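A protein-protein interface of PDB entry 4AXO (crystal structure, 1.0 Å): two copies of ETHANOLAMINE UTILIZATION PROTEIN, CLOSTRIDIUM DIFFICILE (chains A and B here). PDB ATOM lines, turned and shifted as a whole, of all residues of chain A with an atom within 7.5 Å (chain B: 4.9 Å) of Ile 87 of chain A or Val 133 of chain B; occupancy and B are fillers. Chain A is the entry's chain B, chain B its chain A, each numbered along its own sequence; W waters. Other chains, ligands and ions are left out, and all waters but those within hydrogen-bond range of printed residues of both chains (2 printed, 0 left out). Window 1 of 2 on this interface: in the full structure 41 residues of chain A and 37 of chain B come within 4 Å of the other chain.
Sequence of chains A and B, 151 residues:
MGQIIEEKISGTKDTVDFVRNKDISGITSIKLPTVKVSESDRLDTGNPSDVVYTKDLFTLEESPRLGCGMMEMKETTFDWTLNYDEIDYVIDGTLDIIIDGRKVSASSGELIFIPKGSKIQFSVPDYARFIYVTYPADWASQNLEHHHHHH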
ATOM      1  N   LEU A  66     -29.158 -20.725  27.291  1.00  0.00           N
ATOM      2  CA  LEU A  66     -28.168 -21.749  26.982  1.00  0.00           C
ATOM      3  C   LEU A  66     -27.153 -21.187  26.026  1.00  0.00           C
ATOM      4  O   LEU A  66     -27.489 -20.676  24.972  1.00  0.00           O
ATOM      5  CB  LEU A  66     -28.745 -22.997  26.315  1.00  0.00           C
ATOM      6  CG  LEU A  66     -29.583 -23.906  27.216  1.00  0.00           C
ATOM      7  CD1 LEU A  66     -30.177 -25.033  26.400  1.00  0.00           C
ATOM      8  CD2 LEU A  66     -28.770 -24.460  28.368  1.00  0.00           C
ATOM      9  N   GLY A  67     -25.890 -21.295  26.376  1.00  0.00           N
ATOM     10  CA  GLY A  67     -24.802 -20.991  25.471  1.00  0.00           C
ATOM     11  C   GLY A  67     -24.421 -22.270  24.726  1.00  0.00           C
ATOM     12  O   GLY A  67     -24.522 -23.356  25.316  1.00  0.00           O
ATOM     13  N   GLY A  69     -21.453 -23.733  21.664  1.00  0.00           N
ATOM     14  CA  GLY A  69     -20.455 -23.490  20.667  1.00  0.00           C
ATOM     15  C   GLY A  69     -19.576 -24.702  20.426  1.00  0.00           C
ATOM     16  O   GLY A  69     -19.783 -25.773  20.977  1.00  0.00           O
ATOM     17  N   LEU A  82     -14.456 -22.151  35.880  1.00  0.00           N
ATOM     18  CA  LEU A  82     -15.818 -22.059  35.331  1.00  0.00           C
ATOM     19  C   LEU A  82     -16.762 -21.656  36.437  1.00  0.00           C
ATOM     20  O   LEU A  82     -17.176 -22.507  37.232  1.00  0.00           O
ATOM     21  CB  LEU A  82     -16.299 -23.398  34.728  1.00  0.00           C
ATOM     22  CG  LEU A  82     -15.568 -23.892  33.486  1.00  0.00           C
ATOM     23  CD1 LEU A  82     -14.260 -24.574  33.810  1.00  0.00           C
ATOM     24  CD2 LEU A  82     -16.466 -24.891  32.739  1.00  0.00           C
ATOM     25  N   TYR A  84     -19.789 -21.151  35.816  1.00  0.00           N
ATOM     26  CA  TYR A  84     -20.946 -21.502  34.984  1.00  0.00           C
ATOM     27  C   TYR A  84     -20.902 -23.026  34.868  1.00  0.00           C
ATOM     28  O   TYR A  84     -19.857 -23.638  35.093  1.00  0.00           O
ATOM     29  CB  TYR A  84     -20.914 -20.800  33.610  1.00  0.00           C
ATOM     30  CG  TYR A  84     -19.636 -21.000  32.820  1.00  0.00           C
ATOM     31  CD1 TYR A  84     -18.551 -20.165  33.022  1.00  0.00           C
ATOM     32  CD2 TYR A  84     -19.504 -22.018  31.899  1.00  0.00           C
ATOM     33  CE1 TYR A  84     -17.371 -20.327  32.332  1.00  0.00           C
ATOM     34  CE2 TYR A  84     -18.326 -22.194  31.184  1.00  0.00           C
ATOM     35  CZ  TYR A  84     -17.255 -21.347  31.425  1.00  0.00           C
ATOM     36  OH  TYR A  84     -16.049 -21.458  30.775  1.00  0.00           O
ATOM     37  N   ASP A  85     -22.034 -23.628  34.531  1.00  0.00           N
ATOM     38  CA  ASP A  85     -22.110 -25.064  34.277  1.00  0.00           C
ATOM     39  C   ASP A  85     -21.849 -25.340  32.797  1.00  0.00           C
ATOM     40  O   ASP A  85     -22.207 -24.545  31.941  1.00  0.00           O
ATOM     41  CB  ASP A  85     -23.517 -25.576  34.626  1.00  0.00           C
ATOM     42  CG  ASP A  85     -23.840 -25.439  36.063  1.00  0.00           C
ATOM     43  OD1 ASP A  85     -23.427 -26.303  36.870  1.00  0.00           O
ATOM     44  OD2 ASP A  85     -24.522 -24.447  36.428  1.00  0.00           O
ATOM     45  N   GLU A  86     -21.248 -26.504  32.514  1.00  0.00           N
ATOM     46  CA  GLU A  86     -20.926 -26.880  31.147  1.00  0.00           C
ATOM     47  C   GLU A  86     -21.098 -28.368  30.914  1.00  0.00           C
ATOM     48  O   GLU A  86     -20.691 -29.194  31.737  1.00  0.00           O
ATOM     49  CB  GLU A  86     -19.482 -26.460  30.848  1.00  0.00           C
ATOM     50  CG  GLU A  86     -19.010 -26.835  29.421  1.00  0.00           C
ATOM     51  CD  GLU A  86     -17.756 -26.146  29.065  1.00  0.00           C
ATOM     52  OE1 GLU A  86     -17.758 -24.916  29.061  1.00  0.00           O
ATOM     53  OE2 GLU A  86     -16.741 -26.784  28.852  1.00  0.00           O
ATOM     54  N   ILE A  87     -21.663 -28.700  29.754  1.00  0.00           N
ATOM     55  CA  ILE A  87     -21.703 -30.059  29.187  1.00  0.00           C
ATOM     56  C   ILE A  87     -20.908 -30.040  27.898  1.00  0.00           C
ATOM     57  O   ILE A  87     -21.164 -29.194  27.051  1.00  0.00           O
ATOM     58  CB  ILE A  87     -23.164 -30.531  28.860  1.00  0.00           C
ATOM     59  CG1 ILE A  87     -23.979 -30.798  30.133  1.00  0.00           C
ATOM     60  CG2 ILE A  87     -23.155 -31.764  27.951  1.00  0.00           C
ATOM     61  CD1 ILE A  87     -23.708 -32.159  30.789  1.00  0.00           C
ATOM     62  N   ASP A  88     -19.974 -30.985  27.747  1.00  0.00           N
ATOM     63  CA  ASP A  88     -19.209 -31.145  26.526  1.00  0.00           C
ATOM     64  C   ASP A  88     -19.503 -32.502  25.906  1.00  0.00           C
ATOM     65  O   ASP A  88     -19.497 -33.527  26.576  1.00  0.00           O
ATOM     66  CB  ASP A  88     -17.717 -31.068  26.831  1.00  0.00           C
ATOM     67  CG  ASP A  88     -17.333 -29.727  27.443  1.00  0.00           C
ATOM     68  OD1 ASP A  88     -17.735 -28.693  26.899  1.00  0.00           O
ATOM     69  OD2 ASP A  88     -16.644 -29.713  28.480  1.00  0.00           O
ATOM     70  N   TYR A  89     -19.757 -32.505  24.591  1.00  0.00           N
ATOM     71  CA  TYR A  89     -19.885 -33.737  23.812  1.00  0.00           C
ATOM     72  C   TYR A  89     -18.654 -33.796  22.911  1.00  0.00           C
ATOM     73  O   TYR A  89     -18.449 -32.913  22.073  1.00  0.00           O
ATOM     74  CB  TYR A  89     -21.182 -33.768  22.960  1.00  0.00           C
ATOM     75  CG  TYR A  89     -21.356 -35.073  22.213  1.00  0.00           C
ATOM     76  CD1 TYR A  89     -20.655 -35.343  21.042  1.00  0.00           C
ATOM     77  CD2 TYR A  89     -22.231 -36.067  22.651  1.00  0.00           C
ATOM     78  CE1 TYR A  89     -20.749 -36.578  20.387  1.00  0.00           C
ATOM     79  CE2 TYR A  89     -22.345 -37.264  21.993  1.00  0.00           C
ATOM     80  CZ  TYR A  89     -21.607 -37.536  20.851  1.00  0.00           C
ATOM     81  OH  TYR A  89     -21.742 -38.747  20.231  1.00  0.00           O
ATOM     82  N   VAL A  90     -17.820 -34.819  23.107  1.00  0.00           N
ATOM     83  CA  VAL A  90     -16.565 -34.936  22.368  1.00  0.00           C
ATOM     84  C   VAL A  90     -16.826 -35.613  21.040  1.00  0.00           C
ATOM     85  O   VAL A  90     -17.276 -36.757  20.973  1.00  0.00           O
ATOM     86  CB  VAL A  90     -15.496 -35.638  23.196  1.00  0.00           C
ATOM     87  CG1 VAL A  90     -14.187 -35.749  22.422  1.00  0.00           C
ATOM     88  CG2 VAL A  90     -15.278 -34.902  24.515  1.00  0.00           C
ATOM     89  N   LEU A 111     -19.097 -37.910  26.860  1.00  0.00           N
ATOM     90  CA  LEU A 111     -19.559 -36.657  27.416  1.00  0.00           C
ATOM     91  C   LEU A 111     -18.819 -36.279  28.694  1.00  0.00           C
ATOM     92  O   LEU A 111     -18.439 -37.169  29.453  1.00  0.00           O
ATOM     93  CB  LEU A 111     -21.052 -36.881  27.724  1.00  0.00           C
ATOM     94  CG  LEU A 111     -21.870 -35.692  28.217  1.00  0.00           C
ATOM     95  CD1 LEU A 111     -23.194 -35.690  27.662  1.00  0.00           C
ATOM     96  CD2 LEU A 111     -21.810 -35.867  29.760  1.00  0.00           C
ATOM     97  N   ILE A 112     -18.671 -34.986  28.945  1.00  0.00           N
ATOM     98  CA  ILE A 112     -18.203 -34.466  30.213  1.00  0.00           C
ATOM     99  C   ILE A 112     -19.212 -33.443  30.750  1.00  0.00           C
ATOM    100  O   ILE A 112     -19.732 -32.629  30.004  1.00  0.00           O
ATOM    101  CB  ILE A 112     -16.797 -33.839  29.996  1.00  0.00           C
ATOM    102  CG1 ILE A 112     -15.730 -34.980  30.024  1.00  0.00           C
ATOM    103  CG2 ILE A 112     -16.551 -32.636  30.966  1.00  0.00           C
ATOM    104  CD1 ILE A 112     -14.354 -34.496  29.751  1.00  0.00           C
ATOM    105  N   PHE A 113     -19.468 -33.479  32.036  1.00  0.00           N
ATOM    106  CA  PHE A 113     -20.193 -32.439  32.782  1.00  0.00           C
ATOM    107  C   PHE A 113     -19.216 -31.783  33.767  1.00  0.00           C
ATOM    108  O   PHE A 113     -18.521 -32.475  34.531  1.00  0.00           O
ATOM    109  CB  PHE A 113     -21.360 -33.049  33.573  1.00  0.00           C
ATOM    110  CG  PHE A 113     -21.956 -32.109  34.581  1.00  0.00           C
ATOM    111  CD1 PHE A 113     -22.557 -30.932  34.197  1.00  0.00           C
ATOM    112  CD2 PHE A 113     -21.858 -32.377  35.923  1.00  0.00           C
ATOM    113  CE1 PHE A 113     -23.055 -30.030  35.134  1.00  0.00           C
ATOM    114  CE2 PHE A 113     -22.371 -31.470  36.854  1.00  0.00           C
ATOM    115  CZ  PHE A 113     -22.993 -30.308  36.442  1.00  0.00           C
ATOM    116  N   ILE A 114     -19.204 -30.459  33.767  1.00  0.00           N
ATOM    117  CA  ILE A 114     -18.421 -29.653  34.697  1.00  0.00           C
ATOM    118  C   ILE A 114     -19.378 -28.714  35.444  1.00  0.00           C
ATOM    119  O   ILE A 114     -19.973 -27.826  34.858  1.00  0.00           O
ATOM    120  CB  ILE A 114     -17.336 -28.817  33.988  1.00  0.00           C
ATOM    121  CG1 ILE A 114     -16.418 -29.675  33.141  1.00  0.00           C
ATOM    122  CG2 ILE A 114     -16.574 -27.969  35.003  1.00  0.00           C
ATOM    123  CD1 ILE A 114     -15.589 -28.913  32.148  1.00  0.00           C
ATOM    124  N   PRO A 115     -19.522 -28.902  36.765  1.00  0.00           N
ATOM    125  CA  PRO A 115     -20.419 -28.011  37.507  1.00  0.00           C
ATOM    126  C   PRO A 115     -19.824 -26.647  37.714  1.00  0.00           C
ATOM    127  O   PRO A 115     -18.604 -26.448  37.831  1.00  0.00           O
ATOM    128  CB  PRO A 115     -20.625 -28.738  38.846  1.00  0.00           C
ATOM    129  CG  PRO A 115     -19.441 -29.558  38.996  1.00  0.00           C
ATOM    130  CD  PRO A 115     -18.991 -29.989  37.616  1.00  0.00           C
ATOM    131  N   PHE A 130     -15.010 -30.557  20.233  1.00  0.00           N
ATOM    132  CA  PHE A 130     -16.171 -30.843  21.061  1.00  0.00           C
ATOM    133  C   PHE A 130     -17.152 -29.682  21.033  1.00  0.00           C
ATOM    134  O   PHE A 130     -16.768 -28.531  20.936  1.00  0.00           O
ATOM    135  CB  PHE A 130     -15.760 -31.211  22.509  1.00  0.00           C
ATOM    136  CG  PHE A 130     -14.916 -30.207  23.242  1.00  0.00           C
ATOM    137  CD1 PHE A 130     -13.526 -30.197  23.106  1.00  0.00           C
ATOM    138  CD2 PHE A 130     -15.481 -29.335  24.161  1.00  0.00           C
ATOM    139  CE1 PHE A 130     -12.740 -29.336  23.848  1.00  0.00           C
ATOM    140  CE2 PHE A 130     -14.685 -28.500  24.922  1.00  0.00           C
ATOM    141  CZ  PHE A 130     -13.325 -28.520  24.762  1.00  0.00           C
ATOM    142  N   ILE A 131     -18.436 -30.016  21.181  1.00  0.00           N
ATOM    143  CA  ILE A 131     -19.484 -29.050  21.462  1.00  0.00           C
ATOM    144  C   ILE A 131     -19.504 -28.789  22.964  1.00  0.00           C
ATOM    145  O   ILE A 131     -19.392 -29.730  23.752  1.00  0.00           O
ATOM    146  CB  ILE A 131     -20.901 -29.680  21.048  1.00  0.00           C
ATOM    147  CG1 ILE A 131     -21.121 -29.621  19.542  1.00  0.00           C
ATOM    148  CG2 ILE A 131     -22.073 -29.005  21.760  1.00  0.00           C
ATOM    149  CD1 ILE A 131     -21.399 -28.192  19.060  1.00  0.00           C
ATOM    150  N   TYR A 132     -19.700 -27.534  23.344  1.00  0.00           N
ATOM    151  CA  TYR A 132     -19.998 -27.159  24.704  1.00  0.00           C
ATOM    152  C   TYR A 132     -21.394 -26.526  24.762  1.00  0.00           C
ATOM    153  O   TYR A 132     -21.828 -25.823  23.825  1.00  0.00           O
ATOM    154  CB  TYR A 132     -18.968 -26.194  25.291  1.00  0.00           C
ATOM    155  CG  TYR A 132     -18.710 -24.939  24.512  1.00  0.00           C
ATOM    156  CD1 TYR A 132     -19.480 -23.810  24.673  1.00  0.00           C
ATOM    157  CD2 TYR A 132     -17.684 -24.904  23.573  1.00  0.00           C
ATOM    158  CE1 TYR A 132     -19.198 -22.634  23.918  1.00  0.00           C
ATOM    159  CE2 TYR A 132     -17.403 -23.786  22.839  1.00  0.00           C
ATOM    160  CZ  TYR A 132     -18.159 -22.655  23.006  1.00  0.00           C
ATOM    161  OH  TYR A 132     -17.845 -21.566  22.232  1.00  0.00           O
ATOM    162  N   VAL A 133     -22.070 -26.769  25.885  1.00  0.00           N
ATOM    163  CA  VAL A 133     -23.338 -26.140  26.235  1.00  0.00           C
ATOM    164  C   VAL A 133     -23.158 -25.570  27.639  1.00  0.00           C
ATOM    165  O   VAL A 133     -22.685 -26.290  28.525  1.00  0.00           O
ATOM    166  CB  VAL A 133     -24.516 -27.117  26.182  1.00  0.00           C
ATOM    167  CG1 VAL A 133     -25.823 -26.392  26.563  1.00  0.00           C
ATOM    168  CG2 VAL A 133     -24.663 -27.744  24.809  1.00  0.00           C
ATOM    169  N   THR A 134     -23.507 -24.301  27.841  1.00  0.00           N
ATOM    170  CA  THR A 134     -23.302 -23.639  29.115  1.00  0.00           C
ATOM    171  C   THR A 134     -24.577 -23.005  29.641  1.00  0.00           C
ATOM    172  O   THR A 134     -25.473 -22.606  28.907  1.00  0.00           O
ATOM    173  CB  THR A 134     -22.218 -22.550  29.017  1.00  0.00           C
ATOM    174  OG1 THR A 134     -22.652 -21.492  28.167  1.00  0.00           O
ATOM    175  CG2 THR A 134     -20.920 -23.095  28.521  1.00  0.00           C
ATOM    176  N   TYR A 135     -24.586 -22.821  30.958  1.00  0.00           N
ATOM    177  CA  TYR A 135     -25.523 -21.904  31.612  1.00  0.00           C
ATOM    178  C   TYR A 135     -24.760 -21.128  32.674  1.00  0.00           C
ATOM    179  O   TYR A 135     -24.123 -21.759  33.517  1.00  0.00           O
ATOM    180  CB  TYR A 135     -26.707 -22.632  32.290  1.00  0.00           C
ATOM    181  CG  TYR A 135     -27.570 -21.609  32.998  1.00  0.00           C
ATOM    182  CD1 TYR A 135     -28.478 -20.848  32.307  1.00  0.00           C
ATOM    183  CD2 TYR A 135     -27.424 -21.328  34.354  1.00  0.00           C
ATOM    184  CE1 TYR A 135     -29.172 -19.825  32.928  1.00  0.00           C
ATOM    185  CE2 TYR A 135     -28.124 -20.300  34.969  1.00  0.00           C
ATOM    186  CZ  TYR A 135     -28.996 -19.566  34.255  1.00  0.00           C
ATOM    187  OH  TYR A 135     -29.712 -18.547  34.840  1.00  0.00           O
ATOM    188  N   PHE B  58     -28.297 -37.288  35.088  1.00  0.00           N
ATOM    189  CA  PHE B  58     -27.839 -36.566  36.283  1.00  0.00           C
ATOM    190  C   PHE B  58     -29.010 -36.339  37.210  1.00  0.00           C
ATOM    191  O   PHE B  58     -30.080 -35.913  36.761  1.00  0.00           O
ATOM    192  CB  PHE B  58     -27.225 -35.208  35.905  1.00  0.00           C
ATOM    193  CG  PHE B  58     -26.007 -35.339  35.043  1.00  0.00           C
ATOM    194  CD1 PHE B  58     -26.113 -35.431  33.653  1.00  0.00           C
ATOM    195  CD2 PHE B  58     -24.763 -35.455  35.596  1.00  0.00           C
ATOM    196  CE1 PHE B  58     -25.012 -35.613  32.865  1.00  0.00           C
ATOM    197  CE2 PHE B  58     -23.639 -35.609  34.799  1.00  0.00           C
ATOM    198  CZ  PHE B  58     -23.772 -35.694  33.424  1.00  0.00           C
ATOM    199  N   LEU B  66     -28.217 -27.317  34.796  1.00  0.00           N
ATOM    200  CA  LEU B  66     -28.352 -27.966  33.491  1.00  0.00           C
ATOM    201  C   LEU B  66     -28.970 -29.356  33.652  1.00  0.00           C
ATOM    202  O   LEU B  66     -28.549 -30.163  34.461  1.00  0.00           O
ATOM    203  CB  LEU B  66     -27.047 -28.180  32.768  1.00  0.00           C
ATOM    204  CG  LEU B  66     -26.371 -26.924  32.238  1.00  0.00           C
ATOM    205  CD1 LEU B  66     -24.988 -27.256  31.615  1.00  0.00           C
ATOM    206  CD2 LEU B  66     -27.233 -26.248  31.183  1.00  0.00           C
ATOM    207  N   GLY B  67     -29.987 -29.634  32.878  1.00  0.00           N
ATOM    208  CA  GLY B  67     -30.465 -30.995  32.764  1.00  0.00           C
ATOM    209  C   GLY B  67     -29.738 -31.681  31.617  1.00  0.00           C
ATOM    210  O   GLY B  67     -29.361 -31.045  30.636  1.00  0.00           O
ATOM    211  N   CYS B  68     -29.549 -32.983  31.716  1.00  0.00           N
ATOM    212  CA  CYS B  68     -28.983 -33.731  30.591  1.00  0.00           C
ATOM    213  C   CYS B  68     -29.427 -35.169  30.624  1.00  0.00           C
ATOM    214  O   CYS B  68     -29.329 -35.822  31.690  1.00  0.00           O
ATOM    215  CB  CYS B  68     -27.463 -33.623  30.606  1.00  0.00           C
ATOM    216  SG  CYS B  68     -26.620 -34.527  29.311  1.00  0.00           S
ATOM    217  N   ASP B  85     -35.417 -24.365  27.834  1.00  0.00           N
ATOM    218  CA  ASP B  85     -34.596 -24.338  26.631  1.00  0.00           C
ATOM    219  C   ASP B  85     -33.898 -25.693  26.470  1.00  0.00           C
ATOM    220  O   ASP B  85     -33.547 -26.310  27.473  1.00  0.00           O
ATOM    221  CB  ASP B  85     -33.543 -23.231  26.726  1.00  0.00           C
ATOM    222  CG  ASP B  85     -34.141 -21.864  26.823  1.00  0.00           C
ATOM    223  OD1 ASP B  85     -34.567 -21.362  25.770  1.00  0.00           O
ATOM    224  OD2 ASP B  85     -34.187 -21.320  27.938  1.00  0.00           O
ATOM    225  N   GLU B  86     -33.679 -26.112  25.226  1.00  0.00           N
ATOM    226  CA  GLU B  86     -33.109 -27.421  24.945  1.00  0.00           C
ATOM    227  C   GLU B  86     -32.143 -27.372  23.789  1.00  0.00           C
ATOM    228  O   GLU B  86     -32.436 -26.770  22.752  1.00  0.00           O
ATOM    229  CB  GLU B  86     -34.252 -28.401  24.655  1.00  0.00           C
ATOM    230  CG  GLU B  86     -33.787 -29.773  24.204  1.00  0.00           C
ATOM    231  CD  GLU B  86     -34.927 -30.735  24.242  1.00  0.00           C
ATOM    232  OE1 GLU B  86     -35.327 -31.042  25.382  1.00  0.00           O
ATOM    233  OE2 GLU B  86     -35.460 -31.128  23.191  1.00  0.00           O
ATOM    234  N   ILE B  87     -31.028 -28.081  23.939  1.00  0.00           N
ATOM    235  CA  ILE B  87     -30.107 -28.416  22.844  1.00  0.00           C
ATOM    236  C   ILE B  87     -30.125 -29.927  22.706  1.00  0.00           C
ATOM    237  O   ILE B  87     -29.860 -30.629  23.684  1.00  0.00           O
ATOM    238  CB  ILE B  87     -28.612 -27.976  23.140  1.00  0.00           C
ATOM    239  CG1 ILE B  87     -28.401 -26.455  23.095  1.00  0.00           C
ATOM    240  CG2 ILE B  87     -27.632 -28.679  22.206  1.00  0.00           C
ATOM    241  CD1 ILE B  87     -28.352 -25.816  21.708  1.00  0.00           C
ATOM    242  N   ILE B 131     -28.748 -36.885  22.729  1.00  0.00           N
ATOM    243  CA  ILE B 131     -28.595 -36.238  24.011  1.00  0.00           C
ATOM    244  C   ILE B 131     -29.442 -34.971  24.018  1.00  0.00           C
ATOM    245  O   ILE B 131     -29.427 -34.236  23.023  1.00  0.00           O
ATOM    246  CB  ILE B 131     -27.062 -35.829  24.184  1.00  0.00           C
ATOM    247  CG1 ILE B 131     -26.199 -37.034  24.550  1.00  0.00           C
ATOM    248  CG2 ILE B 131     -26.887 -34.725  25.236  1.00  0.00           C
ATOM    249  CD1 ILE B 131     -26.418 -37.522  26.005  1.00  0.00           C
ATOM    250  N   TYR B 132     -30.105 -34.697  25.124  1.00  0.00           N
ATOM    251  CA  TYR B 132     -30.735 -33.402  25.359  1.00  0.00           C
ATOM    252  C   TYR B 132     -30.004 -32.730  26.522  1.00  0.00           C
ATOM    253  O   TYR B 132     -29.624 -33.389  27.512  1.00  0.00           O
ATOM    254  CB  TYR B 132     -32.252 -33.519  25.622  1.00  0.00           C
ATOM    255  CG  TYR B 132     -32.664 -34.411  26.758  1.00  0.00           C
ATOM    256  CD1 TYR B 132     -32.799 -33.949  28.060  1.00  0.00           C
ATOM    257  CD2 TYR B 132     -32.966 -35.752  26.491  1.00  0.00           C
ATOM    258  CE1 TYR B 132     -33.206 -34.805  29.072  1.00  0.00           C
ATOM    259  CE2 TYR B 132     -33.385 -36.604  27.501  1.00  0.00           C
ATOM    260  CZ  TYR B 132     -33.522 -36.126  28.781  1.00  0.00           C
ATOM    261  OH  TYR B 132     -33.941 -37.040  29.743  1.00  0.00           O
ATOM    262  N   VAL B 133     -29.775 -31.442  26.393  1.00  0.00           N
ATOM    263  CA  VAL B 133     -29.257 -30.589  27.459  1.00  0.00           C
ATOM    264  C   VAL B 133     -30.280 -29.471  27.628  1.00  0.00           C
ATOM    265  O   VAL B 133     -30.677 -28.847  26.641  1.00  0.00           O
ATOM    266  CB  VAL B 133     -27.853 -29.996  27.143  1.00  0.00           C
ATOM    267  CG1 VAL B 133     -27.405 -29.118  28.312  1.00  0.00           C
ATOM    268  CG2 VAL B 133     -26.877 -31.109  26.856  1.00  0.00           C
ATOM    269  N   THR B 134     -30.721 -29.228  28.855  1.00  0.00           N
ATOM    270  CA  THR B 134     -31.797 -28.299  29.110  1.00  0.00           C
ATOM    271  C   THR B 134     -31.453 -27.301  30.194  1.00  0.00           C
ATOM    272  O   THR B 134     -30.595 -27.539  31.047  1.00  0.00           O
ATOM    273  CB  THR B 134     -33.074 -29.048  29.506  1.00  0.00           C
ATOM    274  OG1 THR B 134     -32.817 -29.738  30.722  1.00  0.00           O
ATOM    275  CG2 THR B 134     -33.519 -30.009  28.435  1.00  0.00           C
ATOM    276  N   TYR B 135     -32.181 -26.184  30.185  1.00  0.00           N
ATOM    277  CA  TYR B 135     -32.170 -25.266  31.305  1.00  0.00           C
ATOM    278  C   TYR B 135     -33.576 -24.734  31.509  1.00  0.00           C
ATOM    279  O   TYR B 135     -34.170 -24.241  30.562  1.00  0.00           O
ATOM    280  CB  TYR B 135     -31.236 -24.053  31.100  1.00  0.00           C
ATOM    281  CG  TYR B 135     -31.369 -23.119  32.266  1.00  0.00           C
ATOM    282  CD1 TYR B 135     -30.690 -23.369  33.445  1.00  0.00           C
ATOM    283  CD2 TYR B 135     -32.239 -22.018  32.239  1.00  0.00           C
ATOM    284  CE1 TYR B 135     -30.875 -22.602  34.551  1.00  0.00           C
ATOM    285  CE2 TYR B 135     -32.439 -21.224  33.350  1.00  0.00           C
ATOM    286  CZ  TYR B 135     -31.756 -21.523  34.507  1.00  0.00           C
ATOM    287  OH  TYR B 135     -31.950 -20.729  35.616  1.00  0.00           O
HETATM  288  O   HOH W   1     -25.898 -27.827  36.650  1.00  0.00           O
HETATM  289  O   HOH W   2     -31.587 -20.116  25.599  1.00  0.00           O
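OH of Tyr 135 of chain A lies within hydrogen-bond range of OH of Tyr 135 of chain B, 3.2 Å away.
N of Asp 85 of chain B lies within hydrogen-bond range of O of Tyr 135 of chain B, at 3.0 Å. O of Tyr 132 of chain B sits close to SG of Cys 68 of chain B (3.7 Å). N of Asp 85 of chain A sits at hydrogen-bond distance from O of Tyr 135 of chain A, 3.0 Å away. O of Ile 87 of chain B is in hydrogen-bond range of N of Val 133 of chain B, at 2.8 Å. O of Glu 86 of chain A sits at hydrogen-bond distance from N of Ile 114 of chain A (2.8 Å). N of Val 133 of chain A is in hydrogen-bond range of O of Ile 87 of chain A, 2.8 Å away.
Among the printed residues, merely in contact across the chains: Phe 113 of chain A with Phe 58 of chain B, Val 133 of chain A with Val 133 of chain B, Leu 66 of chain A with Leu 66 of chain B, Leu 66 of chain A with Tyr 135 of chain B, Asp 85 of chain A with Leu 66 of chain B, Leu 66 of chain A with Asp 85 of chain B, Tyr 135 of chain A with Leu 66 of chain B, Leu 66 of chain A with Glu 86 of chain B, Leu 66 of chain A with Val 133 of chain B, Glu 86 of chain A with Leu 66 of chain B, Ile 87 of chain A with Val 133 of chain B, Ile 87 of chain A with Leu 66 of chain B, Val 133 of chain A with Leu 66 of chain B and Leu 111 of chain A with Cys 68 of chain B.
Printed residues of chain B within 4 Å of Ile 87 of chain A: Leu 66 and Val 133. Of the printed residues of chain A, Val 133 of chain B touches Leu 66, Ile 87 and Val 133. Of the printed residues of chain A, Cys 68 of chain B touches Leu 111. Of the printed residues of chain B, Glu 86 of chain A touches Leu 66 (3.9 Å). Of the printed residues of chain A, Leu 66 of chain B touches Leu 66, Asp 85, Glu 86, Ile 87, Val 133 and Tyr 135. Of the printed residues of chain B, Tyr 135 of chain A touches Leu 66 and Tyr 135. Printed residues of chain B within 4 Å of Leu 66 of chain A: Leu 66 (3.7 Å), Asp 85 (3.8 Å), Glu 86 (3.8 Å), Val 133 (3.9 Å) and Tyr 135 (3.7 Å). Tyr 84 of chain A touches none of the printed residues of chain B. The nearest printed residue of chain B that does not touch Ile 87 of chain A is Cys 68 of chain B (4.03 Å). The nearest printed residue of chain A that does not touch Val 133 of chain B is Leu 111 of chain A (5.9 Å). The nearest printed residue of chain A that does not touch Phe 58 of chain B is Leu 111 of chain A (4.2 Å).
Hydrophobic or aromatic side chains of chain B that line the printed part of chain A: Phe 58, Leu 66, Val 133 and Tyr 135. Of the 22 printed residues of chain A, 8 touch a printed residue of chain B. Printed residues of chain A that touch a printed residue of chain B: Leu 66, Asp 85, Glu 86, Ile 87, Leu 111, Phe 113, Val 133 and Tyr 135. Along chain A the printed residues that touch a printed residue of chain B span positions 66 to 135. Among the printed residues, no Asp or Glu carboxylate lies within 4 Å of a Lys or Arg side-chain nitrogen of the other chain.
Leu 66 of chain A touches its own counterpart, Leu 66 of chain B. Leu 66 of chain A touches Glu 86 of chain B, and with the chains exchanged Glu 86 of chain A touches Leu 66 of chain B. Leu 66 of chain A touches Val 133 of chain B, and with the chains exchanged Val 133 of chain A touches Leu 66 of chain B. Ile 87 of chain A touches Val 133 of chain B, but with the chains exchanged Val 133 of chain A does not touch Ile 87 of chain B (4.1 Å). Of the 15 pairs that touch across the chains among the printed residues, 11 have their exchanged pair printed and touching as well.
Water W1 lies within hydrogen-bond range of OD1 of Asp 85 of chain A and N of Leu 66 of chain B. Water W2 lies within hydrogen-bond range of N of Leu 66 of chain A (3.0 Å) and OD1 of Asp 85 of chain B (3.2 Å).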
